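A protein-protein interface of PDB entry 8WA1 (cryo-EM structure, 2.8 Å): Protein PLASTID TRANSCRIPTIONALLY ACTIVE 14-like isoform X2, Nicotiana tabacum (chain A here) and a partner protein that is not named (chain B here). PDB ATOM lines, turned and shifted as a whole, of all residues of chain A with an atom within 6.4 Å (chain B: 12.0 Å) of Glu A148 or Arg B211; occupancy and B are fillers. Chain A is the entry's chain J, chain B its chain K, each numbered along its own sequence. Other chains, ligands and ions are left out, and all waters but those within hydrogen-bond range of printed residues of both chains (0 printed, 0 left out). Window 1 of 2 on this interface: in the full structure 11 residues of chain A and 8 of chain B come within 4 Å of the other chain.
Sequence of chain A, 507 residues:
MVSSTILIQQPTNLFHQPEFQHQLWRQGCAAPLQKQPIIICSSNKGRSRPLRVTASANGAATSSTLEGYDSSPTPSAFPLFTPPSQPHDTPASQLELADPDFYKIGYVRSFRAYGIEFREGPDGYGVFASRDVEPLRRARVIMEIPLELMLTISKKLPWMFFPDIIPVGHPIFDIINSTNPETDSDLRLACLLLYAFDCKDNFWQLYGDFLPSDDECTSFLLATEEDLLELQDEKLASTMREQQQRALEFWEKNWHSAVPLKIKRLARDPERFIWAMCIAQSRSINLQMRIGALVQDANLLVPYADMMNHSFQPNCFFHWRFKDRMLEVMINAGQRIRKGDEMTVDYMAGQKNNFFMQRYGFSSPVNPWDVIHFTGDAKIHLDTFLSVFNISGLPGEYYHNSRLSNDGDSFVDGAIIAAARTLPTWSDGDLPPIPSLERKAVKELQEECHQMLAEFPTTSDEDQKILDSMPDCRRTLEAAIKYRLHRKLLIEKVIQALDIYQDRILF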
ATOM      1  N   ARG A 109      -4.389   3.108 -17.629  1.00  0.00           N
ATOM      2  CA  ARG A 109      -5.580   3.075 -18.473  1.00  0.00           C
ATOM      3  C   ARG A 109      -5.571   4.210 -19.481  1.00  0.00           C
ATOM      4  O   ARG A 109      -6.637   4.564 -19.989  1.00  0.00           O
ATOM      5  CB  ARG A 109      -6.851   3.065 -17.632  1.00  0.00           C
ATOM      6  CG  ARG A 109      -7.076   1.735 -16.937  1.00  0.00           C
ATOM      7  CD  ARG A 109      -8.373   1.726 -16.154  1.00  0.00           C
ATOM      8  NE  ARG A 109      -8.580   0.469 -15.443  1.00  0.00           N
ATOM      9  CZ  ARG A 109      -8.112   0.207 -14.226  1.00  0.00           C
ATOM     10  NH1 ARG A 109      -7.399   1.114 -13.571  1.00  0.00           N
ATOM     11  NH2 ARG A 109      -8.354  -0.968 -13.664  1.00  0.00           N
ATOM     12  N   SER A 110      -4.405   4.816 -19.713  1.00  0.00           N
ATOM     13  CA  SER A 110      -4.239   5.897 -20.709  1.00  0.00           C
ATOM     14  C   SER A 110      -4.594   7.322 -20.297  1.00  0.00           C
ATOM     15  O   SER A 110      -4.539   8.226 -21.128  1.00  0.00           O
ATOM     16  CB  SER A 110      -4.844   5.548 -22.081  1.00  0.00           C
ATOM     17  OG  SER A 110      -4.259   4.372 -22.611  1.00  0.00           O
ATOM     18  N   ILE A 145      -8.405  12.722 -20.795  1.00  0.00           N
ATOM     19  CA  ILE A 145      -9.183  11.729 -20.068  1.00  0.00           C
ATOM     20  C   ILE A 145      -9.947  10.881 -21.078  1.00  0.00           C
ATOM     21  O   ILE A 145     -10.825  11.395 -21.776  1.00  0.00           O
ATOM     22  CB  ILE A 145     -10.149  12.381 -19.066  1.00  0.00           C
ATOM     23  CG1 ILE A 145      -9.381  13.328 -18.143  1.00  0.00           C
ATOM     24  CG2 ILE A 145     -10.874  11.318 -18.261  1.00  0.00           C
ATOM     25  CD1 ILE A 145     -10.264  14.185 -17.269  1.00  0.00           C
ATOM     26  N   PRO A 146      -9.655   9.588 -21.192  1.00  0.00           N
ATOM     27  CA  PRO A 146     -10.357   8.753 -22.172  1.00  0.00           C
ATOM     28  C   PRO A 146     -11.822   8.559 -21.810  1.00  0.00           C
ATOM     29  O   PRO A 146     -12.248   8.754 -20.669  1.00  0.00           O
ATOM     30  CB  PRO A 146      -9.597   7.423 -22.119  1.00  0.00           C
ATOM     31  CG  PRO A 146      -8.276   7.754 -21.497  1.00  0.00           C
ATOM     32  CD  PRO A 146      -8.560   8.861 -20.534  1.00  0.00           C
ATOM     33  N   LEU A 147     -12.601   8.168 -22.820  1.00  0.00           N
ATOM     34  CA  LEU A 147     -14.025   7.926 -22.635  1.00  0.00           C
ATOM     35  C   LEU A 147     -14.313   6.608 -21.927  1.00  0.00           C
ATOM     36  O   LEU A 147     -15.376   6.470 -21.311  1.00  0.00           O
ATOM     37  CB  LEU A 147     -14.741   7.949 -23.989  1.00  0.00           C
ATOM     38  CG  LEU A 147     -16.267   7.851 -23.987  1.00  0.00           C
ATOM     39  CD1 LEU A 147     -16.879   9.012 -23.218  1.00  0.00           C
ATOM     40  CD2 LEU A 147     -16.805   7.801 -25.407  1.00  0.00           C
ATOM     41  N   GLU A 148     -13.390   5.649 -21.981  1.00  0.00           N
ATOM     42  CA  GLU A 148     -13.616   4.344 -21.373  1.00  0.00           C
ATOM     43  C   GLU A 148     -13.496   4.361 -19.855  1.00  0.00           C
ATOM     44  O   GLU A 148     -13.733   3.327 -19.221  1.00  0.00           O
ATOM     45  CB  GLU A 148     -12.641   3.318 -21.957  1.00  0.00           C
ATOM     46  CG  GLU A 148     -11.182   3.731 -21.877  1.00  0.00           C
ATOM     47  CD  GLU A 148     -10.251   2.683 -22.448  1.00  0.00           C
ATOM     48  OE1 GLU A 148     -10.748   1.724 -23.076  1.00  0.00           O
ATOM     49  OE2 GLU A 148      -9.021   2.815 -22.270  1.00  0.00           O
ATOM     50  N   LEU A 149     -13.137   5.497 -19.258  1.00  0.00           N
ATOM     51  CA  LEU A 149     -13.081   5.640 -17.809  1.00  0.00           C
ATOM     52  C   LEU A 149     -14.218   6.496 -17.267  1.00  0.00           C
ATOM     53  O   LEU A 149     -14.242   6.793 -16.070  1.00  0.00           O
ATOM     54  CB  LEU A 149     -11.736   6.235 -17.378  1.00  0.00           C
ATOM     55  CG  LEU A 149     -10.459   5.408 -17.545  1.00  0.00           C
ATOM     56  CD1 LEU A 149      -9.939   5.457 -18.973  1.00  0.00           C
ATOM     57  CD2 LEU A 149      -9.391   5.882 -16.572  1.00  0.00           C
ATOM     58  N   MET A 150     -15.166   6.884 -18.116  1.00  0.00           N
ATOM     59  CA  MET A 150     -16.214   7.823 -17.755  1.00  0.00           C
ATOM     60  C   MET A 150     -17.570   7.132 -17.758  1.00  0.00           C
ATOM     61  O   MET A 150     -17.744   6.054 -18.332  1.00  0.00           O
ATOM     62  CB  MET A 150     -16.238   9.014 -18.722  1.00  0.00           C
ATOM     63  CG  MET A 150     -14.945   9.813 -18.761  1.00  0.00           C
ATOM     64  SD  MET A 150     -14.771  10.760 -20.284  1.00  0.00           S
ATOM     65  CE  MET A 150     -16.396  11.496 -20.410  1.00  0.00           C
ATOM     66  N   PRO A 163     -20.361   4.737 -22.840  1.00  0.00           N
ATOM     67  CA  PRO A 163     -19.635   3.765 -22.020  1.00  0.00           C
ATOM     68  C   PRO A 163     -20.588   2.668 -21.581  1.00  0.00           C
ATOM     69  O   PRO A 163     -20.987   2.615 -20.416  1.00  0.00           O
ATOM     70  CB  PRO A 163     -19.102   4.604 -20.845  1.00  0.00           C
ATOM     71  CG  PRO A 163     -19.229   6.029 -21.300  1.00  0.00           C
ATOM     72  CD  PRO A 163     -20.441   6.042 -22.166  1.00  0.00           C
ATOM     73  N   ASN A 202     -13.964  -2.603 -13.725  1.00  0.00           N
ATOM     74  CA  ASN A 202     -14.327  -1.234 -14.050  1.00  0.00           C
ATOM     75  C   ASN A 202     -13.404  -0.271 -13.315  1.00  0.00           C
ATOM     76  O   ASN A 202     -13.000  -0.520 -12.175  1.00  0.00           O
ATOM     77  CB  ASN A 202     -15.787  -0.946 -13.683  1.00  0.00           C
ATOM     78  CG  ASN A 202     -16.319   0.314 -14.345  1.00  0.00           C
ATOM     79  OD1 ASN A 202     -15.573   1.255 -14.614  1.00  0.00           O
ATOM     80  ND2 ASN A 202     -17.619   0.335 -14.611  1.00  0.00           N
ATOM     81  N   PHE A 203     -13.073   0.834 -13.985  1.00  0.00           N
ATOM     82  CA  PHE A 203     -12.174   1.816 -13.390  1.00  0.00           C
ATOM     83  C   PHE A 203     -12.797   2.469 -12.163  1.00  0.00           C
ATOM     84  O   PHE A 203     -12.089   2.836 -11.217  1.00  0.00           O
ATOM     85  CB  PHE A 203     -11.791   2.873 -14.425  1.00  0.00           C
ATOM     86  CG  PHE A 203     -10.909   3.957 -13.882  1.00  0.00           C
ATOM     87  CD1 PHE A 203      -9.568   3.717 -13.639  1.00  0.00           C
ATOM     88  CD2 PHE A 203     -11.419   5.215 -13.614  1.00  0.00           C
ATOM     89  CE1 PHE A 203      -8.752   4.710 -13.137  1.00  0.00           C
ATOM     90  CE2 PHE A 203     -10.609   6.213 -13.113  1.00  0.00           C
ATOM     91  CZ  PHE A 203      -9.273   5.960 -12.874  1.00  0.00           C
ATOM     92  N   LYS A 323     -11.988  12.764 -32.222  1.00  0.00           N
ATOM     93  CA  LYS A 323     -11.177  11.781 -32.936  1.00  0.00           C
ATOM     94  C   LYS A 323     -10.592  10.743 -31.987  1.00  0.00           C
ATOM     95  O   LYS A 323     -10.711   9.536 -32.229  1.00  0.00           O
ATOM     96  CB  LYS A 323     -10.066  12.475 -33.721  1.00  0.00           C
ATOM     97  CG  LYS A 323     -10.519  13.062 -35.047  1.00  0.00           C
ATOM     98  CD  LYS A 323      -9.334  13.517 -35.881  1.00  0.00           C
ATOM     99  CE  LYS A 323      -9.779  14.005 -37.250  1.00  0.00           C
ATOM    100  NZ  LYS A 323     -10.517  12.953 -38.005  1.00  0.00           N
ATOM    101  N   ASP A 324      -9.963  11.185 -30.902  1.00  0.00           N
ATOM    102  CA  ASP A 324      -9.423  10.275 -29.903  1.00  0.00           C
ATOM    103  C   ASP A 324     -10.457   9.861 -28.868  1.00  0.00           C
ATOM    104  O   ASP A 324     -10.157   9.008 -28.026  1.00  0.00           O
ATOM    105  CB  ASP A 324      -8.219  10.906 -29.199  1.00  0.00           C
ATOM    106  CG  ASP A 324      -6.967  10.881 -30.052  1.00  0.00           C
ATOM    107  OD1 ASP A 324      -7.024  10.334 -31.173  1.00  0.00           O
ATOM    108  OD2 ASP A 324      -5.928  11.406 -29.601  1.00  0.00           O
ATOM    109  N   ARG A 325     -11.656  10.438 -28.915  1.00  0.00           N
ATOM    110  CA  ARG A 325     -12.739  10.122 -27.987  1.00  0.00           C
ATOM    111  C   ARG A 325     -12.280  10.306 -26.541  1.00  0.00           C
ATOM    112  O   ARG A 325     -12.426   9.428 -25.689  1.00  0.00           O
ATOM    113  CB  ARG A 325     -13.267   8.706 -28.233  1.00  0.00           C
ATOM    114  CG  ARG A 325     -13.633   8.438 -29.685  1.00  0.00           C
ATOM    115  CD  ARG A 325     -15.123   8.190 -29.850  1.00  0.00           C
ATOM    116  NE  ARG A 325     -15.509   6.859 -29.393  1.00  0.00           N
ATOM    117  CZ  ARG A 325     -15.610   5.798 -30.186  1.00  0.00           C
ATOM    118  NH1 ARG A 325     -15.355   5.912 -31.483  1.00  0.00           N
ATOM    119  NH2 ARG A 325     -15.967   4.624 -29.686  1.00  0.00           N
ATOM    120  N   MET A 326     -11.708  11.479 -26.280  1.00  0.00           N
ATOM    121  CA  MET A 326     -11.198  11.828 -24.964  1.00  0.00           C
ATOM    122  C   MET A 326     -11.655  13.230 -24.587  1.00  0.00           C
ATOM    123  O   MET A 326     -11.831  14.096 -25.447  1.00  0.00           O
ATOM    124  CB  MET A 326      -9.663  11.763 -24.910  1.00  0.00           C
ATOM    125  CG  MET A 326      -9.073  10.405 -25.240  1.00  0.00           C
ATOM    126  SD  MET A 326      -7.306  10.324 -24.889  1.00  0.00           S
ATOM    127  CE  MET A 326      -6.707  11.714 -25.846  1.00  0.00           C
ATOM    128  N   PRO B 205     -11.664  -9.696 -29.634  1.00  0.00           N
ATOM    129  CA  PRO B 205     -12.847  -8.838 -29.755  1.00  0.00           C
ATOM    130  C   PRO B 205     -12.685  -7.836 -30.883  1.00  0.00           C
ATOM    131  O   PRO B 205     -11.575  -7.345 -31.137  1.00  0.00           O
ATOM    132  CB  PRO B 205     -12.913  -8.137 -28.391  1.00  0.00           C
ATOM    133  CG  PRO B 205     -11.508  -8.153 -27.899  1.00  0.00           C
ATOM    134  CD  PRO B 205     -10.926  -9.449 -28.384  1.00  0.00           C
ATOM    135  N   PRO B 206     -13.767  -7.520 -31.591  1.00  0.00           N
ATOM    136  CA  PRO B 206     -13.682  -6.534 -32.677  1.00  0.00           C
ATOM    137  C   PRO B 206     -13.329  -5.154 -32.141  1.00  0.00           C
ATOM    138  O   PRO B 206     -13.799  -4.741 -31.079  1.00  0.00           O
ATOM    139  CB  PRO B 206     -15.086  -6.559 -33.291  1.00  0.00           C
ATOM    140  CG  PRO B 206     -15.674  -7.865 -32.857  1.00  0.00           C
ATOM    141  CD  PRO B 206     -15.103  -8.129 -31.503  1.00  0.00           C
ATOM    142  N   ILE B 207     -12.492  -4.441 -32.888  1.00  0.00           N
ATOM    143  CA  ILE B 207     -12.038  -3.112 -32.495  1.00  0.00           C
ATOM    144  C   ILE B 207     -12.926  -2.080 -33.181  1.00  0.00           C
ATOM    145  O   ILE B 207     -12.873  -1.913 -34.402  1.00  0.00           O
ATOM    146  CB  ILE B 207     -10.562  -2.897 -32.846  1.00  0.00           C
ATOM    147  CG1 ILE B 207      -9.703  -3.993 -32.215  1.00  0.00           C
ATOM    148  CG2 ILE B 207     -10.101  -1.528 -32.377  1.00  0.00           C
ATOM    149  CD1 ILE B 207      -8.233  -3.858 -32.518  1.00  0.00           C
ATOM    150  N   ASP B 208     -13.745  -1.386 -32.391  1.00  0.00           N
ATOM    151  CA  ASP B 208     -14.593  -0.310 -32.889  1.00  0.00           C
ATOM    152  C   ASP B 208     -14.281   1.023 -32.224  1.00  0.00           C
ATOM    153  O   ASP B 208     -15.079   1.961 -32.330  1.00  0.00           O
ATOM    154  CB  ASP B 208     -16.072  -0.660 -32.688  1.00  0.00           C
ATOM    155  CG  ASP B 208     -16.743  -1.099 -33.973  1.00  0.00           C
ATOM    156  OD1 ASP B 208     -16.116  -0.970 -35.045  1.00  0.00           O
ATOM    157  OD2 ASP B 208     -17.898  -1.570 -33.910  1.00  0.00           O
ATOM    158  N   ALA B 209     -13.144   1.132 -31.548  1.00  0.00           N
ATOM    159  CA  ALA B 209     -12.772   2.349 -30.841  1.00  0.00           C
ATOM    160  C   ALA B 209     -11.268   2.530 -30.971  1.00  0.00           C
ATOM    161  O   ALA B 209     -10.545   1.571 -31.281  1.00  0.00           O
ATOM    162  CB  ALA B 209     -13.195   2.287 -29.363  1.00  0.00           C
ATOM    163  N   PRO B 210     -10.763   3.750 -30.764  1.00  0.00           N
ATOM    164  CA  PRO B 210      -9.301   3.937 -30.800  1.00  0.00           C
ATOM    165  C   PRO B 210      -8.563   3.072 -29.791  1.00  0.00           C
ATOM    166  O   PRO B 210      -7.714   2.263 -30.178  1.00  0.00           O
ATOM    167  CB  PRO B 210      -9.140   5.436 -30.512  1.00  0.00           C
ATOM    168  CG  PRO B 210     -10.420   6.044 -30.976  1.00  0.00           C
ATOM    169  CD  PRO B 210     -11.483   5.032 -30.663  1.00  0.00           C
ATOM    170  N   ARG B 211      -8.879   3.202 -28.503  1.00  0.00           N
ATOM    171  CA  ARG B 211      -8.211   2.433 -27.461  1.00  0.00           C
ATOM    172  C   ARG B 211      -8.983   1.177 -27.077  1.00  0.00           C
ATOM    173  O   ARG B 211      -8.893   0.728 -25.929  1.00  0.00           O
ATOM    174  CB  ARG B 211      -7.972   3.311 -26.233  1.00  0.00           C
ATOM    175  CG  ARG B 211      -9.223   3.983 -25.702  1.00  0.00           C
ATOM    176  CD  ARG B 211      -8.865   5.107 -24.750  1.00  0.00           C
ATOM    177  NE  ARG B 211      -7.937   6.053 -25.362  1.00  0.00           N
ATOM    178  CZ  ARG B 211      -8.302   7.037 -26.176  1.00  0.00           C
ATOM    179  NH1 ARG B 211      -9.581   7.207 -26.482  1.00  0.00           N
ATOM    180  NH2 ARG B 211      -7.389   7.850 -26.688  1.00  0.00           N
ATOM    181  N   ASP B 212      -9.739   0.609 -28.011  1.00  0.00           N
ATOM    182  CA  ASP B 212     -10.468  -0.620 -27.737  1.00  0.00           C
ATOM    183  C   ASP B 212      -9.482  -1.750 -27.445  1.00  0.00           C
ATOM    184  O   ASP B 212      -8.423  -1.828 -28.081  1.00  0.00           O
ATOM    185  CB  ASP B 212     -11.357  -0.982 -28.929  1.00  0.00           C
ATOM    186  CG  ASP B 212     -12.455  -1.961 -28.564  1.00  0.00           C
ATOM    187  OD1 ASP B 212     -13.401  -1.560 -27.854  1.00  0.00           O
ATOM    188  OD2 ASP B 212     -12.373  -3.131 -28.992  1.00  0.00           O
ATOM    189  N   PRO B 213      -9.785  -2.630 -26.491  1.00  0.00           N
ATOM    190  CA  PRO B 213      -8.828  -3.683 -26.128  1.00  0.00           C
ATOM    191  C   PRO B 213      -8.530  -4.610 -27.298  1.00  0.00           C
ATOM    192  O   PRO B 213      -9.390  -4.883 -28.138  1.00  0.00           O
ATOM    193  CB  PRO B 213      -9.536  -4.428 -24.990  1.00  0.00           C
ATOM    194  CG  PRO B 213     -10.492  -3.435 -24.427  1.00  0.00           C
ATOM    195  CD  PRO B 213     -10.952  -2.612 -25.593  1.00  0.00           C
ATOM    196  N   MET B 214      -7.289  -5.093 -27.341  1.00  0.00           N
ATOM    197  CA  MET B 214      -6.838  -6.007 -28.379  1.00  0.00           C
ATOM    198  C   MET B 214      -7.199  -7.459 -28.097  1.00  0.00           C
ATOM    199  O   MET B 214      -7.195  -8.272 -29.027  1.00  0.00           O
ATOM    200  CB  MET B 214      -5.318  -5.896 -28.555  1.00  0.00           C
ATOM    201  CG  MET B 214      -4.845  -4.556 -29.091  1.00  0.00           C
ATOM    202  SD  MET B 214      -5.088  -4.402 -30.868  1.00  0.00           S
ATOM    203  CE  MET B 214      -4.067  -5.746 -31.462  1.00  0.00           C
ATOM    204  N   TYR B 215      -7.511  -7.804 -26.849  1.00  0.00           N
ATOM    205  CA  TYR B 215      -7.784  -9.186 -26.489  1.00  0.00           C
ATOM    206  C   TYR B 215      -8.728  -9.228 -25.299  1.00  0.00           C
ATOM    207  O   TYR B 215      -8.885  -8.242 -24.574  1.00  0.00           O
ATOM    208  CB  TYR B 215      -6.493  -9.946 -26.160  1.00  0.00           C
ATOM    209  CG  TYR B 215      -5.773  -9.439 -24.931  1.00  0.00           C
ATOM    210  CD1 TYR B 215      -4.916  -8.349 -25.004  1.00  0.00           C
ATOM    211  CD2 TYR B 215      -5.948 -10.053 -23.697  1.00  0.00           C
ATOM    212  CE1 TYR B 215      -4.254  -7.883 -23.881  1.00  0.00           C
ATOM    213  CE2 TYR B 215      -5.293  -9.594 -22.571  1.00  0.00           C
ATOM    214  CZ  TYR B 215      -4.447  -8.509 -22.668  1.00  0.00           C
ATOM    215  OH  TYR B 215      -3.792  -8.051 -21.549  1.00  0.00           O
ATOM    216  N   LYS B 216      -9.355 -10.387 -25.108  1.00  0.00           N
ATOM    217  CA  LYS B 216     -10.232 -10.642 -23.974  1.00  0.00           C
ATOM    218  C   LYS B 216      -9.936 -12.034 -23.440  1.00  0.00           C
ATOM    219  O   LYS B 216     -10.014 -13.016 -24.186  1.00  0.00           O
ATOM    220  CB  LYS B 216     -11.707 -10.522 -24.375  1.00  0.00           C
ATOM    221  CG  LYS B 216     -12.679 -10.612 -23.213  1.00  0.00           C
ATOM    222  CD  LYS B 216     -14.113 -10.436 -23.686  1.00  0.00           C
ATOM    223  CE  LYS B 216     -15.083 -10.432 -22.517  1.00  0.00           C
ATOM    224  NZ  LYS B 216     -16.489 -10.239 -22.964  1.00  0.00           N
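NH1 of Arg B211 sits at hydrogen-bond distance from O of Asp A324.
NH2 of Arg B211 sits at hydrogen-bond distance from SD of Met A326 (3.1 Å).
Of chain B, only Arg B211 (3.4 Å) comes within 4 Å of Glu A148.
Of chain A, only Pro A146, Glu A148, Asp A324, Arg A325 and Met A326 come within 4 Å of Arg B211.
Leu A147 touches none of the printed residues of chain B.
No residue of chain B comes within 4 Å of Met A150.
No residue of chain B comes within 4 Å of Pro A163.
Of chain B, only Arg B211 comes within 4 Å of Asp A324.
Arg A325 touches just these residues of chain B: Asp B208 (3.9 Å), Ala B209 (3.6 Å) and Arg B211 (3.7 Å).
Of chain B, only Arg B211 (3.1 Å) comes within 4 Å of Met A326.
Of the printed residues of chain A, Ala B209 touches Arg A325.
Printed residues of chain B within 4 Å of Lys A323: Pro B210.
Of the printed residues of chain A, Pro B210 touches Lys A323 (3.7 Å).
Of the printed residues of chain A, Asp B208 touches Arg A325.
Tyr B215 touches none of the printed residues of chain A.
The nearest printed residue of chain A that does not touch Asp B208 is Lys A323 (8.7 Å).
The backbone carbonyl oxygen of Arg A325 lies within hydrogen-bond range of the backbone NH of Leu A147, 3.1 Å away.
Printed residues of chain B that touch a printed residue of chain A: Asp B208, Ala B209, Pro B210 and Arg B211.
Among the printed residues, 8 pairs touch across the chains.
Among the printed residues, no Asp or Glu carboxylate lies within 4 Å of a Lys or Arg side-chain nitrogen of the other chain.
Among the printed residues, merely in contact across the chains: Pro A146 with Arg B211 (3.6 Å), Glu A148 with Arg B211 (3.4 Å), Lys A323 with Pro B210 (3.7 Å), Arg A325 with Asp B208 (3.9 Å), Arg A325 with Ala B209 (3.6 Å) and Arg A325 with Arg B211 (3.7 Å).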
